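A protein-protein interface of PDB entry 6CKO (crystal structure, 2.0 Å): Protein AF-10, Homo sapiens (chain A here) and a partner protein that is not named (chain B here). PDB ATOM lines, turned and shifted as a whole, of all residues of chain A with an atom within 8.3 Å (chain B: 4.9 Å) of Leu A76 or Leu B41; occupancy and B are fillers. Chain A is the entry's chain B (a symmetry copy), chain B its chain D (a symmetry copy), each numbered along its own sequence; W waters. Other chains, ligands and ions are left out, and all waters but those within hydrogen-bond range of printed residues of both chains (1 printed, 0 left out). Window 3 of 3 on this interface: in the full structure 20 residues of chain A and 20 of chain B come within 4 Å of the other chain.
The side-chain amide oxygen of Asn A73 is in hydrogen-bond range of the side-chain hydroxyl of Ser B38, 2.5 Å away.
NE of Arg B45 is in hydrogen-bond range of O of Leu A76 (3.0 Å).
NH2 of Arg B45 is in hydrogen-bond range of O of Gln A75 (3.2 Å).
The chain-end carboxylate (OXT) of Ser A77 is in salt-bridge range of the guanidinium group (NH2) of Arg B45.
The side-chain hydroxyl (OG) of Ser A77 lies within hydrogen-bond range of the backbone carbonyl oxygen (O) of Ala A74.
CD2 of Leu A69 touches OG of Ser B38, at 3.9 Å.
Leu A72 touches Ser B38 (CD2 to OG, 3.8 Å).
CB of Gln B37 touches ND2 of Asn A73, 3.6 Å away.
Asn A73 touches Leu B41 (O to CD1, 3.3 Å).
Leu B41 touches Leu A76 (CB to CB, 3.8 Å).
Of chain B, only Leu B41 and Arg B45 come within 4 Å of Leu A76.
Leu B41 touches just these residues of chain A: Asn A73 and Leu A76.
No residue of chain A comes within 4 Å of Leu B40.
Of the printed residues of chain A, Arg B45 touches Gln A75 (3.2 Å), Leu A76 (3.0 Å) and Ser A77 (3.1 Å).
Of the printed residues of chain A, Ser B38 touches Leu A69, Leu A72 and Asn A73.
Of the printed residues of chain B, Leu A69 touches Ser B38.
Printed residues of chain B within 4 Å of Ser A77: Arg B45.
The nearest residue of chain B that does not touch Leu A76 is Ser B38 (4.02 Å).
Of the 9 printed residues of chain A, 6 touch a printed residue of chain B.
Water W1 lies within hydrogen-bond range of O of Leu A76 (2.8 Å) and O of Leu B41 (2.8 Å).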
ATOM      1  N   LEU A  69     -13.566 -19.029 -25.247  1.00  0.00           N
ATOM      2  CA  LEU A  69     -13.603 -19.484 -23.850  1.00  0.00           C
ATOM      3  C   LEU A  69     -14.931 -19.177 -23.176  1.00  0.00           C
ATOM      4  O   LEU A  69     -15.466 -20.034 -22.470  1.00  0.00           O
ATOM      5  CB  LEU A  69     -12.432 -18.964 -23.040  1.00  0.00           C
ATOM      6  CG  LEU A  69     -11.064 -19.546 -23.393  1.00  0.00           C
ATOM      7  CD1 LEU A  69     -10.028 -18.952 -22.462  1.00  0.00           C
ATOM      8  CD2 LEU A  69     -11.042 -21.051 -23.307  1.00  0.00           C
ATOM      9  N   GLN A  70     -15.514 -18.014 -23.464  1.00  0.00           N
ATOM     10  CA  GLN A  70     -16.851 -17.669 -22.956  1.00  0.00           C
ATOM     11  C   GLN A  70     -17.858 -18.759 -23.361  1.00  0.00           C
ATOM     12  O   GLN A  70     -18.599 -19.219 -22.516  1.00  0.00           O
ATOM     13  CB  GLN A  70     -17.327 -16.289 -23.404  1.00  0.00           C
ATOM     14  CG  GLN A  70     -16.572 -15.122 -22.765  1.00  0.00           C
ATOM     15  CD  GLN A  70     -17.131 -14.687 -21.404  1.00  0.00           C
ATOM     16  OE1 GLN A  70     -17.842 -15.454 -20.755  1.00  0.00           O
ATOM     17  NE2 GLN A  70     -16.840 -13.426 -20.986  1.00  0.00           N
ATOM     18  N   LEU A  71     -17.817 -19.199 -24.629  1.00  0.00           N
ATOM     19  CA  LEU A  71     -18.719 -20.241 -25.109  1.00  0.00           C
ATOM     20  C   LEU A  71     -18.381 -21.618 -24.496  1.00  0.00           C
ATOM     21  O   LEU A  71     -19.255 -22.392 -24.125  1.00  0.00           O
ATOM     22  CB  LEU A  71     -18.721 -20.283 -26.658  1.00  0.00           C
ATOM     23  CG  LEU A  71     -19.269 -18.990 -27.315  1.00  0.00           C
ATOM     24  CD1 LEU A  71     -18.987 -18.856 -28.811  1.00  0.00           C
ATOM     25  CD2 LEU A  71     -20.770 -18.845 -27.040  1.00  0.00           C
ATOM     26  N   LEU A  72     -17.103 -21.947 -24.464  1.00  0.00           N
ATOM     27  CA  LEU A  72     -16.650 -23.180 -23.808  1.00  0.00           C
ATOM     28  C   LEU A  72     -17.128 -23.269 -22.367  1.00  0.00           C
ATOM     29  O   LEU A  72     -17.655 -24.309 -21.963  1.00  0.00           O
ATOM     30  CB  LEU A  72     -15.127 -23.343 -23.887  1.00  0.00           C
ATOM     31  CG  LEU A  72     -14.539 -24.580 -23.177  1.00  0.00           C
ATOM     32  CD1 LEU A  72     -14.974 -25.884 -23.835  1.00  0.00           C
ATOM     33  CD2 LEU A  72     -13.003 -24.495 -23.137  1.00  0.00           C
ATOM     34  N   ASN A  73     -16.998 -22.180 -21.611  1.00  0.00           N
ATOM     35  CA  ASN A  73     -17.370 -22.194 -20.229  1.00  0.00           C
ATOM     36  C   ASN A  73     -18.860 -22.369 -20.011  1.00  0.00           C
ATOM     37  O   ASN A  73     -19.249 -23.087 -19.087  1.00  0.00           O
ATOM     38  CB  ASN A  73     -16.760 -21.019 -19.417  1.00  0.00           C
ATOM     39  CG  ASN A  73     -15.249 -21.144 -19.342  1.00  0.00           C
ATOM     40  OD1 ASN A  73     -14.700 -22.185 -19.768  1.00  0.00           O
ATOM     41  ND2 ASN A  73     -14.565 -20.103 -18.921  1.00  0.00           N
ATOM     42  N   ALA A  74     -19.667 -21.719 -20.845  1.00  0.00           N
ATOM     43  CA  ALA A  74     -21.116 -21.883 -20.825  1.00  0.00           C
ATOM     44  C   ALA A  74     -21.549 -23.359 -21.128  1.00  0.00           C
ATOM     45  O   ALA A  74     -22.449 -23.923 -20.452  1.00  0.00           O
ATOM     46  CB  ALA A  74     -21.763 -20.907 -21.813  1.00  0.00           C
ATOM     47  N   GLN A  75     -20.886 -23.983 -22.108  1.00  0.00           N
ATOM     48  CA  GLN A  75     -21.109 -25.401 -22.423  1.00  0.00           C
ATOM     49  C   GLN A  75     -20.694 -26.363 -21.312  1.00  0.00           C
ATOM     50  O   GLN A  75     -21.400 -27.321 -21.061  1.00  0.00           O
ATOM     51  CB  GLN A  75     -20.383 -25.793 -23.678  1.00  0.00           C
ATOM     52  CG  GLN A  75     -20.889 -25.040 -24.875  1.00  0.00           C
ATOM     53  CD  GLN A  75     -21.814 -25.834 -25.740  1.00  0.00           C
ATOM     54  OE1 GLN A  75     -22.675 -26.565 -25.250  1.00  0.00           O
ATOM     55  NE2 GLN A  75     -21.598 -25.736 -27.062  1.00  0.00           N
ATOM     56  N   LEU A  76     -19.544 -26.124 -20.686  1.00  0.00           N
ATOM     57  CA  LEU A  76     -19.084 -26.965 -19.584  1.00  0.00           C
ATOM     58  C   LEU A  76     -19.898 -26.819 -18.285  1.00  0.00           C
ATOM     59  O   LEU A  76     -19.914 -27.735 -17.474  1.00  0.00           O
ATOM     60  CB  LEU A  76     -17.608 -26.760 -19.290  1.00  0.00           C
ATOM     61  CG  LEU A  76     -16.617 -27.181 -20.385  1.00  0.00           C
ATOM     62  CD1 LEU A  76     -15.232 -26.666 -20.092  1.00  0.00           C
ATOM     63  CD2 LEU A  76     -16.595 -28.658 -20.603  1.00  0.00           C
ATOM     64  N   SER A  77     -20.570 -25.691 -18.080  1.00  0.00           N
ATOM     65  CA  SER A  77     -21.252 -25.464 -16.823  1.00  0.00           C
ATOM     66  C   SER A  77     -22.390 -26.507 -16.627  1.00  0.00           C
ATOM     67  O   SER A  77     -22.670 -26.937 -15.461  1.00  0.00           O
ATOM     68  CB  SER A  77     -21.812 -24.060 -16.768  1.00  0.00           C
ATOM     69  OG  SER A  77     -22.874 -23.912 -17.689  1.00  0.00           O
ATOM     70  OXT SER A  77     -22.985 -26.974 -17.624  1.00  0.00           O
ATOM     71  N   GLN B  37     -11.847 -20.631 -14.822  1.00  0.00           N
ATOM     72  CA  GLN B  37     -13.195 -21.144 -14.855  1.00  0.00           C
ATOM     73  C   GLN B  37     -13.213 -22.465 -15.724  1.00  0.00           C
ATOM     74  O   GLN B  37     -13.813 -23.441 -15.293  1.00  0.00           O
ATOM     75  CB  GLN B  37     -14.179 -20.057 -15.326  1.00  0.00           C
ATOM     76  CG  GLN B  37     -15.441 -19.797 -14.488  1.00  0.00           C
ATOM     77  CD  GLN B  37     -15.247 -19.637 -12.981  1.00  0.00           C
ATOM     78  OE1 GLN B  37     -14.490 -18.797 -12.485  1.00  0.00           O
ATOM     79  NE2 GLN B  37     -15.966 -20.443 -12.245  1.00  0.00           N
ATOM     80  N   SER B  38     -12.560 -22.482 -16.888  1.00  0.00           N
ATOM     81  CA  SER B  38     -12.527 -23.666 -17.790  1.00  0.00           C
ATOM     82  C   SER B  38     -12.019 -24.902 -17.056  1.00  0.00           C
ATOM     83  O   SER B  38     -12.650 -25.914 -17.103  1.00  0.00           O
ATOM     84  CB  SER B  38     -11.647 -23.477 -19.033  1.00  0.00           C
ATOM     85  OG  SER B  38     -12.223 -22.538 -19.920  1.00  0.00           O
ATOM     86  N   GLN B  39     -10.894 -24.767 -16.352  1.00  0.00           N
ATOM     87  CA  GLN B  39     -10.263 -25.861 -15.600  1.00  0.00           C
ATOM     88  C   GLN B  39     -11.194 -26.365 -14.464  1.00  0.00           C
ATOM     89  O   GLN B  39     -11.402 -27.562 -14.335  1.00  0.00           O
ATOM     90  CB  GLN B  39      -8.924 -25.408 -15.012  1.00  0.00           C
ATOM     91  CG  GLN B  39      -7.861 -25.026 -16.043  1.00  0.00           C
ATOM     92  CD  GLN B  39      -6.723 -24.174 -15.471  1.00  0.00           C
ATOM     93  N   LEU B  40     -11.758 -25.444 -13.684  1.00  0.00           N
ATOM     94  CA  LEU B  40     -12.779 -25.761 -12.645  1.00  0.00           C
ATOM     95  C   LEU B  40     -13.964 -26.522 -13.229  1.00  0.00           C
ATOM     96  O   LEU B  40     -14.332 -27.572 -12.721  1.00  0.00           O
ATOM     97  CB  LEU B  40     -13.303 -24.478 -11.970  1.00  0.00           C
ATOM     98  CG  LEU B  40     -14.599 -24.564 -11.124  1.00  0.00           C
ATOM     99  N   LEU B  41     -14.531 -26.020 -14.335  1.00  0.00           N
ATOM    100  CA  LEU B  41     -15.706 -26.629 -14.900  1.00  0.00           C
ATOM    101  C   LEU B  41     -15.388 -27.988 -15.539  1.00  0.00           C
ATOM    102  O   LEU B  41     -16.179 -28.917 -15.435  1.00  0.00           O
ATOM    103  CB  LEU B  41     -16.405 -25.669 -15.888  1.00  0.00           C
ATOM    104  CG  LEU B  41     -16.955 -24.396 -15.226  1.00  0.00           C
ATOM    105  CD1 LEU B  41     -17.424 -23.477 -16.342  1.00  0.00           C
ATOM    106  CD2 LEU B  41     -18.087 -24.689 -14.232  1.00  0.00           C
ATOM    107  N   LEU B  42     -14.216 -28.109 -16.149  1.00  0.00           N
ATOM    108  CA  LEU B  42     -13.816 -29.404 -16.738  1.00  0.00           C
ATOM    109  C   LEU B  42     -13.663 -30.457 -15.634  1.00  0.00           C
ATOM    110  O   LEU B  42     -14.144 -31.588 -15.745  1.00  0.00           O
ATOM    111  CB  LEU B  42     -12.521 -29.255 -17.536  1.00  0.00           C
ATOM    112  CG  LEU B  42     -11.929 -30.501 -18.165  1.00  0.00           C
ATOM    113  CD1 LEU B  42     -12.920 -31.145 -19.099  1.00  0.00           C
ATOM    114  CD2 LEU B  42     -10.655 -30.174 -18.953  1.00  0.00           C
ATOM    115  N   LYS B  43     -12.993 -30.061 -14.565  1.00  0.00           N
ATOM    116  CA  LYS B  43     -12.752 -30.969 -13.448  1.00  0.00           C
ATOM    117  C   LYS B  43     -14.073 -31.455 -12.897  1.00  0.00           C
ATOM    118  O   LYS B  43     -14.245 -32.674 -12.680  1.00  0.00           O
ATOM    119  CB  LYS B  43     -11.865 -30.308 -12.398  1.00  0.00           C
ATOM    120  CG  LYS B  43     -11.416 -31.262 -11.267  1.00  0.00           C
ATOM    121  N   ALA B  44     -15.048 -30.546 -12.748  1.00  0.00           N
ATOM    122  CA  ALA B  44     -16.404 -30.967 -12.293  1.00  0.00           C
ATOM    123  C   ALA B  44     -17.061 -31.951 -13.283  1.00  0.00           C
ATOM    124  O   ALA B  44     -17.644 -32.940 -12.859  1.00  0.00           O
ATOM    125  CB  ALA B  44     -17.296 -29.754 -11.994  1.00  0.00           C
ATOM    126  N   ARG B  45     -16.904 -31.751 -14.593  1.00  0.00           N
ATOM    127  CA  ARG B  45     -17.446 -32.724 -15.522  1.00  0.00           C
ATOM    128  C   ARG B  45     -16.724 -34.068 -15.358  1.00  0.00           C
ATOM    129  O   ARG B  45     -17.373 -35.112 -15.348  1.00  0.00           O
ATOM    130  CB  ARG B  45     -17.351 -32.266 -16.997  1.00  0.00           C
ATOM    131  CG  ARG B  45     -18.270 -31.136 -17.401  1.00  0.00           C
ATOM    132  CD  ARG B  45     -19.696 -31.626 -17.532  1.00  0.00           C
ATOM    133  NE  ARG B  45     -20.569 -30.564 -18.040  1.00  0.00           N
ATOM    134  CZ  ARG B  45     -21.678 -30.747 -18.737  1.00  0.00           C
ATOM    135  NH1 ARG B  45     -22.106 -31.954 -19.102  1.00  0.00           N
ATOM    136  NH2 ARG B  45     -22.369 -29.693 -19.079  1.00  0.00           N
HETATM  137  O   HOH W   1     -18.925 -28.461 -14.940  1.00  0.00           O
